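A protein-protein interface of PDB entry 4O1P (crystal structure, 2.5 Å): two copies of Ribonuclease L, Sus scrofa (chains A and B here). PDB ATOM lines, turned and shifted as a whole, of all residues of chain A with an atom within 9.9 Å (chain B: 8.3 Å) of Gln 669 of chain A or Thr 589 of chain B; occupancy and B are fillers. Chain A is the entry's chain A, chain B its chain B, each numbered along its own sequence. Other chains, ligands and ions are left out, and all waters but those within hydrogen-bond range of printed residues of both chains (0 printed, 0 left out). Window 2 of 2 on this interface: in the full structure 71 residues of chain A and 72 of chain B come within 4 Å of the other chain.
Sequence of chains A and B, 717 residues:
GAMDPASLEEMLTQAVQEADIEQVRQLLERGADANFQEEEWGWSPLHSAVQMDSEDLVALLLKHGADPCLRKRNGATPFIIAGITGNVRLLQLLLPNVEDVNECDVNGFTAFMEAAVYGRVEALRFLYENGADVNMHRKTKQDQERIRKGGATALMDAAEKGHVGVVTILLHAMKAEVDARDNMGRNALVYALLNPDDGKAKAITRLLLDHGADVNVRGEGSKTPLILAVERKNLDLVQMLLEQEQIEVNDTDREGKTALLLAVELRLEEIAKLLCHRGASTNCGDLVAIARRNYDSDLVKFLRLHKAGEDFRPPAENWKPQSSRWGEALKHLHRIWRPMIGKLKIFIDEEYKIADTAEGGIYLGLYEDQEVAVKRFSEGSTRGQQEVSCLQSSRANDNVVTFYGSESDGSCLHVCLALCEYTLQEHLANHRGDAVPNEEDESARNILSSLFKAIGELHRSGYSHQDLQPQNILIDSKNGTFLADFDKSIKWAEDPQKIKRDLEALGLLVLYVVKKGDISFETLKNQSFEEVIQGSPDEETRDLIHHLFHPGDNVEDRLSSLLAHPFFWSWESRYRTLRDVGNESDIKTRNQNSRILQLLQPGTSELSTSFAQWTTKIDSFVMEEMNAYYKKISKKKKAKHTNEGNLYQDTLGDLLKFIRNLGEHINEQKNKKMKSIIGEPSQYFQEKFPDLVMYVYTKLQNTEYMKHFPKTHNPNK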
ATOM      1  N   GLU A 625      -1.931  20.317  16.583  1.00  0.00           N
ATOM      2  CA  GLU A 625      -1.270  21.500  16.020  1.00  0.00           C
ATOM      3  C   GLU A 625      -2.306  22.459  15.492  1.00  0.00           C
ATOM      4  O   GLU A 625      -2.182  23.675  15.665  1.00  0.00           O
ATOM      5  CB  GLU A 625      -0.329  21.140  14.861  1.00  0.00           C
ATOM      6  CG  GLU A 625       0.893  20.328  15.245  1.00  0.00           C
ATOM      7  CD  GLU A 625       1.724  19.956  14.039  1.00  0.00           C
ATOM      8  OE1 GLU A 625       1.268  20.159  12.899  1.00  0.00           O
ATOM      9  OE2 GLU A 625       2.832  19.421  14.244  1.00  0.00           O
ATOM     10  N   GLU A 664      -4.899  26.108   3.433  1.00  0.00           N
ATOM     11  CA  GLU A 664      -4.161  27.362   3.277  1.00  0.00           C
ATOM     12  C   GLU A 664      -2.755  27.331   3.879  1.00  0.00           C
ATOM     13  O   GLU A 664      -1.862  28.020   3.381  1.00  0.00           O
ATOM     14  CB  GLU A 664      -4.949  28.533   3.876  1.00  0.00           C
ATOM     15  CG  GLU A 664      -6.224  28.874   3.121  1.00  0.00           C
ATOM     16  CD  GLU A 664      -5.972  29.303   1.681  1.00  0.00           C
ATOM     17  OE1 GLU A 664      -5.145  30.224   1.478  1.00  0.00           O
ATOM     18  OE2 GLU A 664      -6.602  28.725   0.759  1.00  0.00           O
ATOM     19  N   HIS A 665      -2.554  26.531   4.925  1.00  0.00           N
ATOM     20  CA  HIS A 665      -1.310  26.572   5.707  1.00  0.00           C
ATOM     21  C   HIS A 665      -0.459  25.294   5.630  1.00  0.00           C
ATOM     22  O   HIS A 665       0.613  25.245   6.215  1.00  0.00           O
ATOM     23  CB  HIS A 665      -1.633  26.902   7.177  1.00  0.00           C
ATOM     24  CG  HIS A 665      -2.442  28.154   7.351  1.00  0.00           C
ATOM     25  ND1 HIS A 665      -2.031  29.382   6.876  1.00  0.00           N
ATOM     26  CD2 HIS A 665      -3.632  28.371   7.959  1.00  0.00           C
ATOM     27  CE1 HIS A 665      -2.938  30.299   7.173  1.00  0.00           C
ATOM     28  NE2 HIS A 665      -3.918  29.714   7.835  1.00  0.00           N
ATOM     29  N   ILE A 666      -0.905  24.288   4.883  1.00  0.00           N
ATOM     30  CA  ILE A 666      -0.219  22.982   4.837  1.00  0.00           C
ATOM     31  C   ILE A 666       1.217  23.020   4.283  1.00  0.00           C
ATOM     32  O   ILE A 666       2.077  22.259   4.737  1.00  0.00           O
ATOM     33  CB  ILE A 666      -1.049  21.921   4.049  1.00  0.00           C
ATOM     34  CG1 ILE A 666      -0.438  20.517   4.157  1.00  0.00           C
ATOM     35  CG2 ILE A 666      -1.208  22.297   2.579  1.00  0.00           C
ATOM     36  CD1 ILE A 666      -0.411  19.978   5.566  1.00  0.00           C
ATOM     37  N   ASN A 667       1.470  23.877   3.293  1.00  0.00           N
ATOM     38  CA  ASN A 667       2.765  23.895   2.602  1.00  0.00           C
ATOM     39  C   ASN A 667       3.812  24.786   3.279  1.00  0.00           C
ATOM     40  O   ASN A 667       4.958  24.852   2.822  1.00  0.00           O
ATOM     41  CB  ASN A 667       2.586  24.317   1.137  1.00  0.00           C
ATOM     42  CG  ASN A 667       1.645  23.394   0.372  1.00  0.00           C
ATOM     43  OD1 ASN A 667       1.991  22.257   0.060  1.00  0.00           O
ATOM     44  ND2 ASN A 667       0.449  23.886   0.063  1.00  0.00           N
ATOM     45  N   GLU A 668       3.425  25.466   4.359  1.00  0.00           N
ATOM     46  CA  GLU A 668       4.352  26.315   5.114  1.00  0.00           C
ATOM     47  C   GLU A 668       5.424  25.479   5.820  1.00  0.00           C
ATOM     48  O   GLU A 668       5.190  24.322   6.182  1.00  0.00           O
ATOM     49  CB  GLU A 668       3.600  27.195   6.117  1.00  0.00           C
ATOM     50  CG  GLU A 668       2.686  28.219   5.454  1.00  0.00           C
ATOM     51  CD  GLU A 668       1.853  29.018   6.441  1.00  0.00           C
ATOM     52  OE1 GLU A 668       2.159  29.000   7.651  1.00  0.00           O
ATOM     53  OE2 GLU A 668       0.879  29.668   6.001  1.00  0.00           O
ATOM     54  N   GLN A 669       6.603  26.083   5.980  1.00  0.00           N
ATOM     55  CA  GLN A 669       7.810  25.392   6.466  1.00  0.00           C
ATOM     56  C   GLN A 669       7.648  24.781   7.862  1.00  0.00           C
ATOM     57  O   GLN A 669       8.109  23.667   8.116  1.00  0.00           O
ATOM     58  CB  GLN A 669       9.020  26.342   6.432  1.00  0.00           C
ATOM     59  CG  GLN A 669       8.877  27.608   7.273  1.00  0.00           C
ATOM     60  CD  GLN A 669       9.958  28.638   6.982  1.00  0.00           C
ATOM     61  OE1 GLN A 669      11.120  28.292   6.758  1.00  0.00           O
ATOM     62  NE2 GLN A 669       9.580  29.917   6.993  1.00  0.00           N
ATOM     63  N   LYS A 670       6.987  25.513   8.756  1.00  0.00           N
ATOM     64  CA  LYS A 670       6.704  25.020  10.109  1.00  0.00           C
ATOM     65  C   LYS A 670       5.929  23.688  10.136  1.00  0.00           C
ATOM     66  O   LYS A 670       6.045  22.930  11.102  1.00  0.00           O
ATOM     67  CB  LYS A 670       5.967  26.085  10.949  1.00  0.00           C
ATOM     68  CG  LYS A 670       6.783  27.322  11.310  1.00  0.00           C
ATOM     69  CD  LYS A 670       6.068  28.214  12.314  1.00  0.00           C
ATOM     70  CE  LYS A 670       4.831  28.871  11.714  1.00  0.00           C
ATOM     71  NZ  LYS A 670       4.204  29.834  12.662  1.00  0.00           N
ATOM     72  N   ASN A 671       5.159  23.406   9.084  1.00  0.00           N
ATOM     73  CA  ASN A 671       4.265  22.241   9.040  1.00  0.00           C
ATOM     74  C   ASN A 671       4.803  21.038   8.247  1.00  0.00           C
ATOM     75  O   ASN A 671       4.024  20.194   7.802  1.00  0.00           O
ATOM     76  CB  ASN A 671       2.898  22.666   8.473  1.00  0.00           C
ATOM     77  CG  ASN A 671       2.132  23.597   9.408  1.00  0.00           C
ATOM     78  OD1 ASN A 671       1.916  23.278  10.576  1.00  0.00           O
ATOM     79  ND2 ASN A 671       1.700  24.742   8.894  1.00  0.00           N
ATOM     80  N   LYS A 672       6.122  20.939   8.094  1.00  0.00           N
ATOM     81  CA  LYS A 672       6.744  19.827   7.339  1.00  0.00           C
ATOM     82  C   LYS A 672       6.270  18.417   7.736  1.00  0.00           C
ATOM     83  O   LYS A 672       6.094  17.557   6.872  1.00  0.00           O
ATOM     84  CB  LYS A 672       8.278  19.873   7.440  1.00  0.00           C
ATOM     85  CG  LYS A 672       9.000  20.102   6.117  1.00  0.00           C
ATOM     86  CD  LYS A 672       9.049  21.570   5.724  1.00  0.00           C
ATOM     87  CE  LYS A 672      10.097  21.832   4.651  1.00  0.00           C
ATOM     88  NZ  LYS A 672      10.272  23.294   4.408  1.00  0.00           N
ATOM     89  N   LYS A 673       6.085  18.178   9.034  1.00  0.00           N
ATOM     90  CA  LYS A 673       5.659  16.859   9.518  1.00  0.00           C
ATOM     91  C   LYS A 673       4.199  16.590   9.170  1.00  0.00           C
ATOM     92  O   LYS A 673       3.852  15.500   8.701  1.00  0.00           O
ATOM     93  CB  LYS A 673       5.853  16.743  11.031  1.00  0.00           C
ATOM     94  CG  LYS A 673       7.294  16.544  11.460  1.00  0.00           C
ATOM     95  CD  LYS A 673       7.459  16.774  12.955  1.00  0.00           C
ATOM     96  CE  LYS A 673       8.925  16.915  13.343  1.00  0.00           C
ATOM     97  NZ  LYS A 673       9.082  17.498  14.705  1.00  0.00           N
ATOM     98  N   MET A 674       3.350  17.587   9.419  1.00  0.00           N
ATOM     99  CA  MET A 674       1.932  17.532   9.045  1.00  0.00           C
ATOM    100  C   MET A 674       1.793  17.115   7.588  1.00  0.00           C
ATOM    101  O   MET A 674       1.137  16.122   7.277  1.00  0.00           O
ATOM    102  CB  MET A 674       1.279  18.897   9.262  1.00  0.00           C
ATOM    103  CG  MET A 674      -0.232  18.902   9.117  1.00  0.00           C
ATOM    104  SD  MET A 674      -0.947  20.351   9.927  1.00  0.00           S
ATOM    105  CE  MET A 674      -0.717  21.630   8.721  1.00  0.00           C
ATOM    106  N   LYS A 675       2.464  17.861   6.714  1.00  0.00           N
ATOM    107  CA  LYS A 675       2.460  17.613   5.268  1.00  0.00           C
ATOM    108  C   LYS A 675       2.821  16.169   4.914  1.00  0.00           C
ATOM    109  O   LYS A 675       2.179  15.555   4.060  1.00  0.00           O
ATOM    110  CB  LYS A 675       3.442  18.572   4.585  1.00  0.00           C
ATOM    111  CG  LYS A 675       3.223  18.782   3.095  1.00  0.00           C
ATOM    112  CD  LYS A 675       4.422  19.500   2.486  1.00  0.00           C
ATOM    113  CE  LYS A 675       4.077  20.228   1.200  1.00  0.00           C
ATOM    114  NZ  LYS A 675       3.857  19.314   0.050  1.00  0.00           N
ATOM    115  N   SER A 676       3.835  15.631   5.589  1.00  0.00           N
ATOM    116  CA  SER A 676       4.340  14.287   5.304  1.00  0.00           C
ATOM    117  C   SER A 676       3.374  13.194   5.744  1.00  0.00           C
ATOM    118  O   SER A 676       3.311  12.135   5.115  1.00  0.00           O
ATOM    119  CB  SER A 676       5.701  14.070   5.979  1.00  0.00           C
ATOM    120  OG  SER A 676       5.581  14.020   7.394  1.00  0.00           O
ATOM    121  N   GLY B 582       0.333  33.881  -4.426  1.00  0.00           N
ATOM    122  CA  GLY B 582       0.419  34.681  -3.198  1.00  0.00           C
ATOM    123  C   GLY B 582       0.290  33.925  -1.876  1.00  0.00           C
ATOM    124  O   GLY B 582       0.408  34.528  -0.808  1.00  0.00           O
ATOM    125  N   ASN B 583       0.051  32.616  -1.944  1.00  0.00           N
ATOM    126  CA  ASN B 583      -0.015  31.760  -0.763  1.00  0.00           C
ATOM    127  C   ASN B 583       1.243  30.911  -0.550  1.00  0.00           C
ATOM    128  O   ASN B 583       1.353  30.212   0.461  1.00  0.00           O
ATOM    129  CB  ASN B 583      -1.223  30.830  -0.850  1.00  0.00           C
ATOM    130  CG  ASN B 583      -1.544  30.177   0.475  1.00  0.00           C
ATOM    131  OD1 ASN B 583      -1.813  30.867   1.445  1.00  0.00           O
ATOM    132  ND2 ASN B 583      -1.491  28.849   0.532  1.00  0.00           N
ATOM    133  N   GLU B 584       2.175  30.952  -1.497  1.00  0.00           N
ATOM    134  CA  GLU B 584       3.484  30.324  -1.316  1.00  0.00           C
ATOM    135  C   GLU B 584       4.158  30.864  -0.047  1.00  0.00           C
ATOM    136  O   GLU B 584       4.153  32.074   0.203  1.00  0.00           O
ATOM    137  CB  GLU B 584       4.367  30.583  -2.540  1.00  0.00           C
ATOM    138  CG  GLU B 584       4.080  29.653  -3.710  1.00  0.00           C
ATOM    139  CD  GLU B 584       4.611  28.247  -3.496  1.00  0.00           C
ATOM    140  OE1 GLU B 584       5.470  28.064  -2.609  1.00  0.00           O
ATOM    141  OE2 GLU B 584       4.169  27.317  -4.216  1.00  0.00           O
ATOM    142  N   SER B 585       4.717  29.972   0.761  1.00  0.00           N
ATOM    143  CA  SER B 585       5.236  30.368   2.080  1.00  0.00           C
ATOM    144  C   SER B 585       6.330  31.431   1.968  1.00  0.00           C
ATOM    145  O   SER B 585       6.394  32.358   2.783  1.00  0.00           O
ATOM    146  CB  SER B 585       5.734  29.148   2.855  1.00  0.00           C
ATOM    147  OG  SER B 585       6.425  28.249   2.006  1.00  0.00           O
ATOM    148  N   ASP B 586       7.160  31.306   0.934  1.00  0.00           N
ATOM    149  CA  ASP B 586       8.256  32.247   0.685  1.00  0.00           C
ATOM    150  C   ASP B 586       7.775  33.648   0.274  1.00  0.00           C
ATOM    151  O   ASP B 586       8.467  34.636   0.515  1.00  0.00           O
ATOM    152  CB  ASP B 586       9.209  31.677  -0.363  1.00  0.00           C
ATOM    153  CG  ASP B 586       9.878  30.383   0.098  1.00  0.00           C
ATOM    154  OD1 ASP B 586      10.398  30.345   1.238  1.00  0.00           O
ATOM    155  OD2 ASP B 586       9.884  29.399  -0.679  1.00  0.00           O
ATOM    156  N   ILE B 587       6.598  33.737  -0.337  1.00  0.00           N
ATOM    157  CA  ILE B 587       5.974  35.037  -0.601  1.00  0.00           C
ATOM    158  C   ILE B 587       5.483  35.682   0.705  1.00  0.00           C
ATOM    159  O   ILE B 587       5.636  36.883   0.897  1.00  0.00           O
ATOM    160  CB  ILE B 587       4.793  34.916  -1.596  1.00  0.00           C
ATOM    161  CG1 ILE B 587       5.296  34.502  -2.997  1.00  0.00           C
ATOM    162  CG2 ILE B 587       3.974  36.205  -1.632  1.00  0.00           C
ATOM    163  CD1 ILE B 587       5.460  35.623  -3.998  1.00  0.00           C
ATOM    164  N   LYS B 588       4.889  34.886   1.591  1.00  0.00           N
ATOM    165  CA  LYS B 588       4.297  35.408   2.832  1.00  0.00           C
ATOM    166  C   LYS B 588       5.359  35.815   3.862  1.00  0.00           C
ATOM    167  O   LYS B 588       5.186  36.814   4.562  1.00  0.00           O
ATOM    168  CB  LYS B 588       3.312  34.391   3.438  1.00  0.00           C
ATOM    169  CG  LYS B 588       2.124  34.074   2.524  1.00  0.00           C
ATOM    170  CD  LYS B 588       0.992  33.345   3.236  1.00  0.00           C
ATOM    171  CE  LYS B 588       1.297  31.872   3.450  1.00  0.00           C
ATOM    172  NZ  LYS B 588       0.067  31.110   3.803  1.00  0.00           N
ATOM    173  N   THR B 589       6.451  35.052   3.942  1.00  0.00           N
ATOM    174  CA  THR B 589       7.602  35.411   4.784  1.00  0.00           C
ATOM    175  C   THR B 589       8.539  36.438   4.120  1.00  0.00           C
ATOM    176  O   THR B 589       9.510  36.880   4.735  1.00  0.00           O
ATOM    177  CB  THR B 589       8.439  34.170   5.175  1.00  0.00           C
ATOM    178  OG1 THR B 589       8.992  33.555   4.004  1.00  0.00           O
ATOM    179  CG2 THR B 589       7.581  33.158   5.940  1.00  0.00           C
ATOM    180  N   ARG B 590       8.240  36.811   2.874  1.00  0.00           N
ATOM    181  CA  ARG B 590       9.058  37.744   2.090  1.00  0.00           C
ATOM    182  C   ARG B 590      10.535  37.321   2.038  1.00  0.00           C
ATOM    183  O   ARG B 590      11.434  38.161   2.107  1.00  0.00           O
ATOM    184  CB  ARG B 590       8.906  39.171   2.632  1.00  0.00           C
ATOM    185  CG  ARG B 590       9.151  40.256   1.590  1.00  0.00           C
ATOM    186  CD  ARG B 590       9.323  41.639   2.209  1.00  0.00           C
ATOM    187  NE  ARG B 590       8.072  42.402   2.290  1.00  0.00           N
ATOM    188  CZ  ARG B 590       7.202  42.370   3.305  1.00  0.00           C
ATOM    189  NH1 ARG B 590       7.408  41.597   4.367  1.00  0.00           N
ATOM    190  NH2 ARG B 590       6.104  43.123   3.256  1.00  0.00           N
ATOM    191  N   ASN B 591      10.766  36.012   1.914  1.00  0.00           N
ATOM    192  CA  ASN B 591      12.114  35.449   1.821  1.00  0.00           C
ATOM    193  C   ASN B 591      12.710  35.746   0.446  1.00  0.00           C
ATOM    194  O   ASN B 591      12.469  35.019  -0.521  1.00  0.00           O
ATOM    195  CB  ASN B 591      12.087  33.935   2.087  1.00  0.00           C
ATOM    196  CG  ASN B 591      13.451  33.272   1.925  1.00  0.00           C
ATOM    197  OD1 ASN B 591      14.490  33.926   1.990  1.00  0.00           O
ATOM    198  ND2 ASN B 591      13.446  31.961   1.719  1.00  0.00           N
ATOM    199  N   GLN B 592      13.506  36.813   0.382  1.00  0.00           N
ATOM    200  CA  GLN B 592      14.030  37.351  -0.881  1.00  0.00           C
ATOM    201  C   GLN B 592      14.960  36.406  -1.664  1.00  0.00           C
ATOM    202  O   GLN B 592      15.104  36.552  -2.876  1.00  0.00           O
ATOM    203  CB  GLN B 592      14.745  38.684  -0.611  1.00  0.00           C
ATOM    204  CG  GLN B 592      13.838  39.815  -0.162  1.00  0.00           C
ATOM    205  CD  GLN B 592      14.608  41.082   0.158  1.00  0.00           C
ATOM    206  OE1 GLN B 592      15.794  41.034   0.494  1.00  0.00           O
ATOM    207  NE2 GLN B 592      13.936  42.223   0.072  1.00  0.00           N
ATOM    208  N   SER B 594      14.482  33.103  -1.877  1.00  0.00           N
ATOM    209  CA  SER B 594      13.708  31.931  -2.288  1.00  0.00           C
ATOM    210  C   SER B 594      13.678  31.794  -3.806  1.00  0.00           C
ATOM    211  O   SER B 594      13.780  32.789  -4.530  1.00  0.00           O
ATOM    212  CB  SER B 594      12.276  32.050  -1.784  1.00  0.00           C
ATOM    213  OG  SER B 594      11.652  33.201  -2.329  1.00  0.00           O
ATOM    214  N   LEU B 597      10.647  33.905  -5.361  1.00  0.00           N
ATOM    215  CA  LEU B 597      10.853  35.341  -5.451  1.00  0.00           C
ATOM    216  C   LEU B 597      11.998  35.671  -6.410  1.00  0.00           C
ATOM    217  O   LEU B 597      12.010  36.787  -6.964  1.00  0.00           O
ATOM    218  CB  LEU B 597      11.081  35.998  -4.077  1.00  0.00           C
ATOM    219  CG  LEU B 597       9.845  36.301  -3.220  1.00  0.00           C
ATOM    220  CD1 LEU B 597      10.247  37.068  -1.972  1.00  0.00           C
ATOM    221  CD2 LEU B 597       8.784  37.095  -3.973  1.00  0.00           C
ATOM    222  N   ASP B 654       4.681  41.120  -2.885  1.00  0.00           N
ATOM    223  CA  ASP B 654       3.731  41.704  -1.933  1.00  0.00           C
ATOM    224  C   ASP B 654       2.371  41.978  -2.548  1.00  0.00           C
ATOM    225  O   ASP B 654       1.361  41.956  -1.839  1.00  0.00           O
ATOM    226  CB  ASP B 654       4.286  42.990  -1.293  1.00  0.00           C
ATOM    227  CG  ASP B 654       5.160  42.707  -0.056  1.00  0.00           C
ATOM    228  OD1 ASP B 654       5.619  41.550   0.115  1.00  0.00           O
ATOM    229  OD2 ASP B 654       5.364  43.646   0.750  1.00  0.00           O
ATOM    230  N   LYS B 657       0.783  38.529  -2.415  1.00  0.00           N
ATOM    231  CA  LYS B 657       0.429  38.378  -1.005  1.00  0.00           C
ATOM    232  C   LYS B 657      -0.853  39.157  -0.705  1.00  0.00           C
ATOM    233  O   LYS B 657      -1.777  38.652  -0.070  1.00  0.00           O
ATOM    234  CB  LYS B 657       1.611  38.858  -0.136  1.00  0.00           C
ATOM    235  CG  LYS B 657       1.396  38.880   1.370  1.00  0.00           C
ATOM    236  CD  LYS B 657       0.830  37.570   1.893  1.00  0.00           C
ATOM    237  CE  LYS B 657       0.755  37.545   3.420  1.00  0.00           C
ATOM    238  NZ  LYS B 657      -0.260  36.568   3.932  1.00  0.00           N
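Of the 14 printed residues of chain A, 4 touch a printed residue of chain B. Printed residues of chain B that touch a printed residue of chain A: Asn 583, Ser 585, Lys 588 and Thr 589. Among the printed residues, 6 pairs touch across the chains.
The side-chain amide oxygen (OD1) of Asn 583 of chain B sits at hydrogen-bond distance from the side-chain amino group (NZ) of Lys 588 of chain B. ND1 of His 665 of chain A is in hydrogen-bond range of OE2 of Glu 668 of chain A (3.1 Å). The backbone carbonyl oxygen (O) of Ser 585 of chain B is in hydrogen-bond range of the side-chain hydroxyl (OG1) of Thr 589 of chain B (3.1 Å). The side-chain amide oxygen (OD1) of Asn 667 of chain A sits close to the side-chain amino group (NZ) of Lys 675 of chain A, at 3.5 Å.
OE2 of Glu 668 of chain A lies within salt-bridge range of NZ of Lys 588 of chain B, at 2.8 Å. The side-chain amide nitrogen of Asn 583 of chain B sits at hydrogen-bond distance from the backbone carbonyl oxygen of Glu 664 of chain A.
Of the printed residues of chain B, Glu 668 of chain A touches Ser 585 and Lys 588. Of the printed residues of chain B, Gln 669 of chain A touches Thr 589. Of the printed residues of chain A, Ser 585 of chain B touches Asn 667 and Glu 668. Of the printed residues of chain A, Lys 588 of chain B touches Glu 664 and Glu 668. The nearest residue of chain A that does not touch Thr 589 of chain B is Glu 668 of chain A (7.0 Å).
No position is printed for both chains. Of the 6 pairs that touch across the chains among the printed residues, none has its exchanged pair printed and touching as well.
Among the printed residues, pairs that only touch across the chains: Glu 664 of chain A with Lys 588 of chain B, Asn 667 of chain A with Ser 585 of chain B, Glu 668 of chain A with Ser 585 of chain B and Gln 669 of chain A with Thr 589 of chain B.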
